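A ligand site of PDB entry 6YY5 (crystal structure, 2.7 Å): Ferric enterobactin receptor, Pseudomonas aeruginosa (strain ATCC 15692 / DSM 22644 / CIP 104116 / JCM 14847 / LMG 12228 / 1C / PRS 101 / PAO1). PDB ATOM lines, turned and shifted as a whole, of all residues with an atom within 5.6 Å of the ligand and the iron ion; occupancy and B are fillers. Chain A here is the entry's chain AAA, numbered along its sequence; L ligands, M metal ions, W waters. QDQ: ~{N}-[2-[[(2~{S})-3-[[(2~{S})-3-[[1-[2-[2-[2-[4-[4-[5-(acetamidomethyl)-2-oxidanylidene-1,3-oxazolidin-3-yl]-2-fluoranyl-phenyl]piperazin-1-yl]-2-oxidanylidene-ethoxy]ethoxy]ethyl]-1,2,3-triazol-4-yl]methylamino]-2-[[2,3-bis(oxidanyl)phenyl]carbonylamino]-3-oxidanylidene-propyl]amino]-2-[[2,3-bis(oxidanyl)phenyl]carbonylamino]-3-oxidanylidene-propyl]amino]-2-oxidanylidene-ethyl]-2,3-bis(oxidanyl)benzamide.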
ATOM      1  N   ARG A 107       1.861  25.319 -22.654  1.00  0.00           N
ATOM      2  CA  ARG A 107       0.424  25.310 -22.293  1.00  0.00           C
ATOM      3  C   ARG A 107      -0.430  25.547 -23.548  1.00  0.00           C
ATOM      4  O   ARG A 107      -1.641  25.731 -23.385  1.00  0.00           O
ATOM      5  CB  ARG A 107       0.103  26.393 -21.258  1.00  0.00           C
ATOM      6  CG  ARG A 107       1.068  26.445 -20.093  1.00  0.00           C
ATOM      7  CD  ARG A 107       1.244  25.088 -19.460  1.00  0.00           C
ATOM      8  NE  ARG A 107       2.401  25.013 -18.582  1.00  0.00           N
ATOM      9  CZ  ARG A 107       2.690  23.951 -17.838  1.00  0.00           C
ATOM     10  NH1 ARG A 107       1.879  22.909 -17.865  1.00  0.00           N
ATOM     11  NH2 ARG A 107       3.797  23.912 -17.103  1.00  0.00           N
ATOM     12  N   LYS A 221      10.157  39.799  -5.375  1.00  0.00           N
ATOM     13  CA  LYS A 221      10.804  40.178  -6.657  1.00  0.00           C
ATOM     14  C   LYS A 221       9.763  40.763  -7.624  1.00  0.00           C
ATOM     15  O   LYS A 221      10.151  41.651  -8.417  1.00  0.00           O
ATOM     16  CB  LYS A 221      11.496  38.964  -7.286  1.00  0.00           C
ATOM     17  CG  LYS A 221      12.772  38.529  -6.577  1.00  0.00           C
ATOM     18  CD  LYS A 221      13.273  37.171  -6.990  1.00  0.00           C
ATOM     19  CE  LYS A 221      14.469  36.716  -6.167  1.00  0.00           C
ATOM     20  NZ  LYS A 221      14.746  35.276  -6.373  1.00  0.00           N
ATOM     21  N   GLN A 222       8.562  40.173  -7.667  1.00  0.00           N
ATOM     22  CA  GLN A 222       7.564  40.407  -8.747  1.00  0.00           C
ATOM     23  C   GLN A 222       6.655  41.588  -8.366  1.00  0.00           C
ATOM     24  O   GLN A 222       5.738  41.929  -9.155  1.00  0.00           O
ATOM     25  CB  GLN A 222       6.738  39.139  -9.047  1.00  0.00           C
ATOM     26  CG  GLN A 222       7.566  37.896  -9.352  1.00  0.00           C
ATOM     27  CD  GLN A 222       8.364  38.003 -10.622  1.00  0.00           C
ATOM     28  OE1 GLN A 222       9.197  37.147 -10.914  1.00  0.00           O
ATOM     29  NE2 GLN A 222       8.150  39.063 -11.381  1.00  0.00           N
ATOM     30  N   GLN A 270       4.631  35.916 -21.119  1.00  0.00           N
ATOM     31  CA  GLN A 270       3.899  34.647 -20.842  1.00  0.00           C
ATOM     32  C   GLN A 270       3.358  34.654 -19.403  1.00  0.00           C
ATOM     33  O   GLN A 270       2.141  34.389 -19.223  1.00  0.00           O
ATOM     34  CB  GLN A 270       4.773  33.418 -21.087  1.00  0.00           C
ATOM     35  CG  GLN A 270       4.044  32.122 -20.759  1.00  0.00           C
ATOM     36  CD  GLN A 270       4.906  30.916 -21.014  1.00  0.00           C
ATOM     37  OE1 GLN A 270       5.089  30.496 -22.152  1.00  0.00           O
ATOM     38  NE2 GLN A 270       5.512  30.417 -19.955  1.00  0.00           N
ATOM     39  N   ASN A 271       4.203  34.906 -18.408  1.00  0.00           N
ATOM     40  CA  ASN A 271       3.833  34.682 -16.983  1.00  0.00           C
ATOM     41  C   ASN A 271       3.470  35.985 -16.293  1.00  0.00           C
ATOM     42  O   ASN A 271       3.273  35.930 -15.064  1.00  0.00           O
ATOM     43  CB  ASN A 271       4.981  34.006 -16.232  1.00  0.00           C
ATOM     44  CG  ASN A 271       5.375  32.760 -16.964  1.00  0.00           C
ATOM     45  OD1 ASN A 271       4.499  31.974 -17.321  1.00  0.00           O
ATOM     46  ND2 ASN A 271       6.626  32.686 -17.386  1.00  0.00           N
ATOM     47  N   ASN A 273       5.550  38.281 -15.551  1.00  0.00           N
ATOM     48  CA  ASN A 273       6.831  38.812 -14.977  1.00  0.00           C
ATOM     49  C   ASN A 273       7.296  39.991 -15.837  1.00  0.00           C
ATOM     50  O   ASN A 273       6.760  40.214 -16.916  1.00  0.00           O
ATOM     51  CB  ASN A 273       7.898  37.718 -14.876  1.00  0.00           C
ATOM     52  CG  ASN A 273       8.035  36.855 -16.117  1.00  0.00           C
ATOM     53  OD1 ASN A 273       7.115  36.752 -16.939  1.00  0.00           O
ATOM     54  ND2 ASN A 273       9.138  36.128 -16.193  1.00  0.00           N
ATOM     55  N   ALA A 326      12.734  28.644 -20.724  1.00  0.00           N
ATOM     56  CA  ALA A 326      12.918  27.946 -19.417  1.00  0.00           C
ATOM     57  C   ALA A 326      12.084  28.613 -18.314  1.00  0.00           C
ATOM     58  O   ALA A 326      12.465  29.715 -17.867  1.00  0.00           O
ATOM     59  CB  ALA A 326      14.381  27.920 -19.015  1.00  0.00           C
ATOM     60  N   GLY A 327      11.133  27.852 -17.754  1.00  0.00           N
ATOM     61  CA  GLY A 327      10.394  28.182 -16.519  1.00  0.00           C
ATOM     62  C   GLY A 327       9.703  29.529 -16.630  1.00  0.00           C
ATOM     63  O   GLY A 327       8.919  29.724 -17.595  1.00  0.00           O
ATOM     64  N   GLY A 328       9.949  30.401 -15.642  1.00  0.00           N
ATOM     65  CA  GLY A 328       9.476  31.796 -15.614  1.00  0.00           C
ATOM     66  C   GLY A 328      10.115  32.646 -16.697  1.00  0.00           C
ATOM     67  O   GLY A 328       9.621  33.763 -16.915  1.00  0.00           O
ATOM     68  N   THR A 329      11.167  32.166 -17.354  1.00  0.00           N
ATOM     69  CA  THR A 329      11.844  32.918 -18.455  1.00  0.00           C
ATOM     70  C   THR A 329      11.249  32.514 -19.810  1.00  0.00           C
ATOM     71  O   THR A 329      11.699  33.104 -20.839  1.00  0.00           O
ATOM     72  CB  THR A 329      13.374  32.779 -18.398  1.00  0.00           C
ATOM     73  OG1 THR A 329      13.795  31.593 -19.082  1.00  0.00           O
ATOM     74  CG2 THR A 329      13.881  32.754 -16.974  1.00  0.00           C
ATOM     75  N   GLU A 389      21.955  22.653 -16.997  1.00  0.00           N
ATOM     76  CA  GLU A 389      21.354  22.729 -15.646  1.00  0.00           C
ATOM     77  C   GLU A 389      20.596  21.421 -15.350  1.00  0.00           C
ATOM     78  O   GLU A 389      20.679  20.923 -14.239  1.00  0.00           O
ATOM     79  CB  GLU A 389      20.459  23.965 -15.547  1.00  0.00           C
ATOM     80  CG  GLU A 389      19.864  24.170 -14.173  1.00  0.00           C
ATOM     81  CD  GLU A 389      19.294  25.557 -13.916  1.00  0.00           C
ATOM     82  OE1 GLU A 389      20.089  26.517 -13.929  1.00  0.00           O
ATOM     83  OE2 GLU A 389      18.071  25.674 -13.741  1.00  0.00           O
ATOM     84  N   TYR A 481      12.193  23.789 -20.533  1.00  0.00           N
ATOM     85  CA  TYR A 481      12.751  23.392 -19.219  1.00  0.00           C
ATOM     86  C   TYR A 481      12.077  24.201 -18.110  1.00  0.00           C
ATOM     87  O   TYR A 481      11.608  25.356 -18.309  1.00  0.00           O
ATOM     88  CB  TYR A 481      14.273  23.512 -19.242  1.00  0.00           C
ATOM     89  CG  TYR A 481      14.953  23.436 -17.892  1.00  0.00           C
ATOM     90  CD1 TYR A 481      15.026  22.244 -17.200  1.00  0.00           C
ATOM     91  CD2 TYR A 481      15.631  24.530 -17.378  1.00  0.00           C
ATOM     92  CE1 TYR A 481      15.717  22.140 -16.016  1.00  0.00           C
ATOM     93  CE2 TYR A 481      16.318  24.450 -16.172  1.00  0.00           C
ATOM     94  CZ  TYR A 481      16.364  23.249 -15.489  1.00  0.00           C
ATOM     95  OH  TYR A 481      17.001  23.167 -14.286  1.00  0.00           O
ATOM     96  N   SER A 482      11.852  23.516 -16.991  1.00  0.00           N
ATOM     97  CA  SER A 482      11.374  24.124 -15.727  1.00  0.00           C
ATOM     98  C   SER A 482      12.171  23.501 -14.588  1.00  0.00           C
ATOM     99  O   SER A 482      12.514  22.309 -14.702  1.00  0.00           O
ATOM    100  CB  SER A 482       9.895  23.926 -15.531  1.00  0.00           C
ATOM    101  OG  SER A 482       9.510  24.134 -14.166  1.00  0.00           O
ATOM    102  N   ARG A 483      12.475  24.312 -13.571  1.00  0.00           N
ATOM    103  CA  ARG A 483      13.137  23.816 -12.324  1.00  0.00           C
ATOM    104  C   ARG A 483      12.114  23.108 -11.432  1.00  0.00           C
ATOM    105  O   ARG A 483      12.536  22.516 -10.436  1.00  0.00           O
ATOM    106  CB  ARG A 483      13.805  24.954 -11.537  1.00  0.00           C
ATOM    107  CG  ARG A 483      14.781  25.794 -12.355  1.00  0.00           C
ATOM    108  CD  ARG A 483      15.464  26.861 -11.514  1.00  0.00           C
ATOM    109  NE  ARG A 483      16.688  27.368 -12.128  1.00  0.00           N
ATOM    110  CZ  ARG A 483      17.015  28.661 -12.251  1.00  0.00           C
ATOM    111  NH1 ARG A 483      16.212  29.605 -11.778  1.00  0.00           N
ATOM    112  NH2 ARG A 483      18.137  29.001 -12.884  1.00  0.00           N
ATOM    113  N   GLY A 484      10.838  23.100 -11.800  1.00  0.00           N
ATOM    114  CA  GLY A 484       9.806  22.365 -11.049  1.00  0.00           C
ATOM    115  C   GLY A 484       8.433  22.971 -11.185  1.00  0.00           C
ATOM    116  O   GLY A 484       7.482  22.204 -11.421  1.00  0.00           O
ATOM    117  N   GLN A 485       8.339  24.306 -11.115  1.00  0.00           N
ATOM    118  CA  GLN A 485       7.051  25.042 -10.906  1.00  0.00           C
ATOM    119  C   GLN A 485       6.044  24.659 -12.004  1.00  0.00           C
ATOM    120  O   GLN A 485       4.827  24.741 -11.755  1.00  0.00           O
ATOM    121  CB  GLN A 485       7.298  26.548 -10.857  1.00  0.00           C
ATOM    122  CG  GLN A 485       6.064  27.390 -10.516  1.00  0.00           C
ATOM    123  CD  GLN A 485       6.427  28.633  -9.673  1.00  0.00           C
ATOM    124  OE1 GLN A 485       5.697  29.041  -8.760  1.00  0.00           O
ATOM    125  NE2 GLN A 485       7.596  29.229  -9.932  1.00  0.00           N
ATOM    126  N   GLY A 486       6.526  24.196 -13.163  1.00  0.00           N
ATOM    127  CA  GLY A 486       5.676  23.842 -14.325  1.00  0.00           C
ATOM    128  C   GLY A 486       5.687  22.356 -14.648  1.00  0.00           C
ATOM    129  O   GLY A 486       5.260  21.983 -15.760  1.00  0.00           O
ATOM    130  N   SER A 491       7.942  18.531  -7.994  1.00  0.00           N
ATOM    131  CA  SER A 491       8.574  19.869  -7.802  1.00  0.00           C
ATOM    132  C   SER A 491       9.957  19.905  -8.470  1.00  0.00           C
ATOM    133  O   SER A 491      10.575  20.983  -8.448  1.00  0.00           O
ATOM    134  CB  SER A 491       8.697  20.181  -6.332  1.00  0.00           C
ATOM    135  OG  SER A 491       7.951  19.259  -5.550  1.00  0.00           O
ATOM    136  N   TYR A 644      -0.142  23.502 -12.831  1.00  0.00           N
ATOM    137  CA  TYR A 644       0.792  22.809 -13.747  1.00  0.00           C
ATOM    138  C   TYR A 644       1.251  21.506 -13.082  1.00  0.00           C
ATOM    139  O   TYR A 644       1.825  20.658 -13.807  1.00  0.00           O
ATOM    140  CB  TYR A 644       1.965  23.714 -14.142  1.00  0.00           C
ATOM    141  CG  TYR A 644       1.586  25.068 -14.697  1.00  0.00           C
ATOM    142  CD1 TYR A 644       0.679  25.197 -15.733  1.00  0.00           C
ATOM    143  CD2 TYR A 644       2.143  26.219 -14.181  1.00  0.00           C
ATOM    144  CE1 TYR A 644       0.298  26.451 -16.216  1.00  0.00           C
ATOM    145  CE2 TYR A 644       1.756  27.474 -14.634  1.00  0.00           C
ATOM    146  CZ  TYR A 644       0.854  27.591 -15.666  1.00  0.00           C
ATOM    147  OH  TYR A 644       0.546  28.830 -16.154  1.00  0.00           O
ATOM    148  N   VAL A 698       1.803  31.680  -9.378  1.00  0.00           N
ATOM    149  CA  VAL A 698       3.242  31.296  -9.296  1.00  0.00           C
ATOM    150  C   VAL A 698       3.875  32.049  -8.124  1.00  0.00           C
ATOM    151  O   VAL A 698       3.173  32.846  -7.452  1.00  0.00           O
ATOM    152  CB  VAL A 698       3.971  31.559 -10.632  1.00  0.00           C
ATOM    153  CG1 VAL A 698       3.351  30.761 -11.763  1.00  0.00           C
ATOM    154  CG2 VAL A 698       4.028  33.041 -10.975  1.00  0.00           C
ATOM    155  N   VAL A 699       5.150  31.763  -7.821  1.00  0.00           N
ATOM    156  CA  VAL A 699       5.893  32.487  -6.736  1.00  0.00           C
ATOM    157  C   VAL A 699       5.801  33.993  -7.017  1.00  0.00           C
ATOM    158  O   VAL A 699       6.311  34.436  -8.070  1.00  0.00           O
ATOM    159  CB  VAL A 699       7.350  32.015  -6.643  1.00  0.00           C
ATOM    160  CG1 VAL A 699       8.131  32.830  -5.632  1.00  0.00           C
ATOM    161  CG2 VAL A 699       7.460  30.525  -6.344  1.00  0.00           C
ATOM    162  N   GLY A 700       5.292  34.762  -6.047  1.00  0.00           N
ATOM    163  CA  GLY A 700       5.255  36.236  -6.100  1.00  0.00           C
ATOM    164  C   GLY A 700       4.139  36.791  -6.986  1.00  0.00           C
ATOM    165  O   GLY A 700       3.948  38.005  -6.947  1.00  0.00           O
ATOM    166  N   ILE A 701       3.478  35.951  -7.812  1.00  0.00           N
ATOM    167  CA  ILE A 701       2.362  36.383  -8.711  1.00  0.00           C
ATOM    168  C   ILE A 701       1.157  35.477  -8.445  1.00  0.00           C
ATOM    169  O   ILE A 701       1.042  34.446  -9.132  1.00  0.00           O
ATOM    170  CB  ILE A 701       2.762  36.377 -10.201  1.00  0.00           C
ATOM    171  CG1 ILE A 701       4.214  36.832 -10.412  1.00  0.00           C
ATOM    172  CG2 ILE A 701       1.773  37.205 -11.004  1.00  0.00           C
ATOM    173  CD1 ILE A 701       4.622  36.878 -11.868  1.00  0.00           C
HETATM  174  C19 QDQ L   1       9.952  35.946  -8.260  1.00  0.00           C
HETATM  175  C20 QDQ L   1       9.943  34.665  -9.035  1.00  0.00           C
HETATM  176  N6  QDQ L   1      11.067  33.809  -8.725  1.00  0.00           N
HETATM  177  C21 QDQ L   1      11.114  32.523  -9.101  1.00  0.00           C
HETATM  178  O5  QDQ L   1      10.189  31.962  -9.694  1.00  0.00           O
HETATM  179  C22 QDQ L   1      12.359  31.728  -8.706  1.00  0.00           C
HETATM  180  C23 QDQ L   1      13.647  32.179  -9.395  1.00  0.00           C
HETATM  181  N7  QDQ L   1      13.492  32.351 -10.832  1.00  0.00           N
HETATM  182  C24 QDQ L   1      13.072  33.491 -11.386  1.00  0.00           C
HETATM  183  O6  QDQ L   1      12.849  34.519 -10.739  1.00  0.00           O
HETATM  184  C25 QDQ L   1      12.824  33.457 -12.883  1.00  0.00           C
HETATM  185  C26 QDQ L   1      11.417  33.983 -13.222  1.00  0.00           C
HETATM  186  N8  QDQ L   1      10.377  33.416 -12.377  1.00  0.00           N
HETATM  187  C27 QDQ L   1       9.109  33.806 -12.452  1.00  0.00           C
HETATM  188  O7  QDQ L   1       8.755  34.742 -13.176  1.00  0.00           O
HETATM  189  C28 QDQ L   1       8.097  33.027 -11.628  1.00  0.00           C
HETATM  190  N9  QDQ L   1       7.841  31.678 -12.112  1.00  0.00           N
HETATM  191  C29 QDQ L   1       6.929  31.419 -13.064  1.00  0.00           C
HETATM  192  O8  QDQ L   1       6.109  32.270 -13.412  1.00  0.00           O
HETATM  193  C30 QDQ L   1       6.918  30.089 -13.726  1.00  0.00           C
HETATM  194  C31 QDQ L   1       5.909  29.839 -14.656  1.00  0.00           C
HETATM  195  C32 QDQ L   1       5.852  28.670 -15.364  1.00  0.00           C
HETATM  196  C33 QDQ L   1       6.792  27.660 -15.123  1.00  0.00           C
HETATM  197  C34 QDQ L   1       7.812  27.865 -14.214  1.00  0.00           C
HETATM  198  O9  QDQ L   1       8.707  26.853 -14.006  1.00  0.00           O
HETATM  199  C35 QDQ L   1       7.885  29.090 -13.514  1.00  0.00           C
HETATM  200  O10 QDQ L   1       8.892  29.215 -12.620  1.00  0.00           O
HETATM  201  N10 QDQ L   1      13.068  32.074 -13.352  1.00  0.00           N
HETATM  202  C36 QDQ L   1      14.258  31.639 -13.903  1.00  0.00           C
HETATM  203  O11 QDQ L   1      15.191  32.410 -14.120  1.00  0.00           O
HETATM  204  C37 QDQ L   1      14.343  30.201 -14.264  1.00  0.00           C
HETATM  205  C38 QDQ L   1      15.457  29.701 -14.946  1.00  0.00           C
HETATM  206  C39 QDQ L   1      15.561  28.381 -15.246  1.00  0.00           C
HETATM  207  C40 QDQ L   1      14.517  27.504 -14.920  1.00  0.00           C
HETATM  208  C41 QDQ L   1      13.357  27.981 -14.302  1.00  0.00           C
HETATM  209  O12 QDQ L   1      12.329  27.147 -13.974  1.00  0.00           O
HETATM  210  C42 QDQ L   1      13.286  29.315 -13.944  1.00  0.00           C
HETATM  211  O13 QDQ L   1      12.135  29.714 -13.343  1.00  0.00           O
HETATM  212  N11 QDQ L   1      12.103  30.318  -8.944  1.00  0.00           N
HETATM  213  C43 QDQ L   1      11.384  29.577  -8.100  1.00  0.00           C
HETATM  214  O14 QDQ L   1      10.858  30.054  -7.083  1.00  0.00           O
HETATM  215  C44 QDQ L   1      11.100  28.175  -8.494  1.00  0.00           C
HETATM  216  C45 QDQ L   1      10.893  27.185  -7.531  1.00  0.00           C
HETATM  217  C46 QDQ L   1      10.545  25.913  -7.877  1.00  0.00           C
HETATM  218  C47 QDQ L   1      10.382  25.588  -9.222  1.00  0.00           C
HETATM  219  C48 QDQ L   1      10.564  26.541 -10.203  1.00  0.00           C
HETATM  220  O15 QDQ L   1      10.379  26.267 -11.542  1.00  0.00           O
HETATM  221  C49 QDQ L   1      10.932  27.844  -9.849  1.00  0.00           C
HETATM  222  O16 QDQ L   1      11.083  28.733 -10.867  1.00  0.00           O
HETATM  223 FE    FE M   1      10.904  28.043 -12.601  1.00  0.00          FE
HETATM  224  O   HOH W   1      13.797  29.568 -10.965  1.00  0.00           O
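The backbone NH (N) of Gln 485 sits at hydrogen-bond distance from the side-chain hydroxyl (OG) of Ser 482 (3.3 Å).
The side-chain hydroxyl (OG) of Ser 482 sits at hydrogen-bond distance from the backbone NH (N) of Gly 484 (2.9 Å).
OG of Ser 482 lies within hydrogen-bond range of N of Gly 486, at 3.1 Å.
The side-chain carboxylate (OE2) of Glu 389 is in salt-bridge range of the guanidinium group (NE) of Arg 483 (2.7 Å).
The side-chain hydroxyl (OG1) of Thr 329 lies within hydrogen-bond range of the backbone carbonyl oxygen (O) of Ala 326, at 2.6 Å.
The backbone carbonyl oxygen of Gly 328 is in hydrogen-bond range of the side-chain amide nitrogen of Asn 273, at 2.5 Å.
The backbone NH (N) of Gly 327 is in hydrogen-bond range of the backbone carbonyl oxygen (O) of Tyr 481, 2.6 Å away.
OH of Tyr 481 sits at hydrogen-bond distance from OE2 of Glu 389.
Residues that only touch the iron ion: Gly 327 (3.95 Å) and Gly 328 (3.96 Å).
The nearest printed residue that does not touch the iron ion is Arg 483 (4.2 Å).
The iron ion is bound by O16 of the ligand, O15 of the ligand, O12 of the ligand, O13 of the ligand and O10 of the ligand.
An oxygen (O9) of the ligand is in hydrogen-bond range of the side-chain hydroxyl (OG) of Ser 482 (2.8 Å).
N of Gln 485 sits close to O15 of the ligand, 2.9 Å away.
A nitrogen (N9) of the ligand lies close to the side-chain amide nitrogen (NE2) of Gln 485 (3.3 Å).
O12 of the ligand lies close to N of Arg 483 (2.9 Å).
The side-chain amide oxygen (OE1) of Gln 222 lies close to an oxygen (O7) of the ligand (3.3 Å).
N of Gly 484 lies close to O15 of the ligand, at 3.2 Å.
The backbone NH (N) of Gly 328 lies close to an oxygen (O13) of the ligand (3.2 Å).
An oxygen (O7) of the ligand is in hydrogen-bond range of the side-chain amide nitrogen (ND2) of Asn 273 (3.3 Å).
Residues that only touch the ligand: Lys 221 (3.5 Å), Asn 271 (3.5 Å), Ala 326 (3.98 Å), Gly 327 (3.3 Å), Thr 329 (3.2 Å), Glu 389 (3.99 Å), Tyr 481 (3.8 Å), Gly 486 (3.5 Å), Val 698 (3.3 Å) and Val 699 (3.5 Å).
Hydrophobic or aromatic side chains that line the ligand: Ala 326, Tyr 481, Val 698 and Val 699.
Within 4 Å of the ligand: Lys 221, Gln 222, Asn 271, Asn 273, Ala 326, Gly 327, Gly 328, Thr 329, Glu 389, Tyr 481, Ser 482, Arg 483, Gly 484, Gln 485, Gly 486, Val 698 and Val 699.
Water W1 bridges NH1 of Arg 483 (2.5 Å) and N11 of the ligand (2.7 Å).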
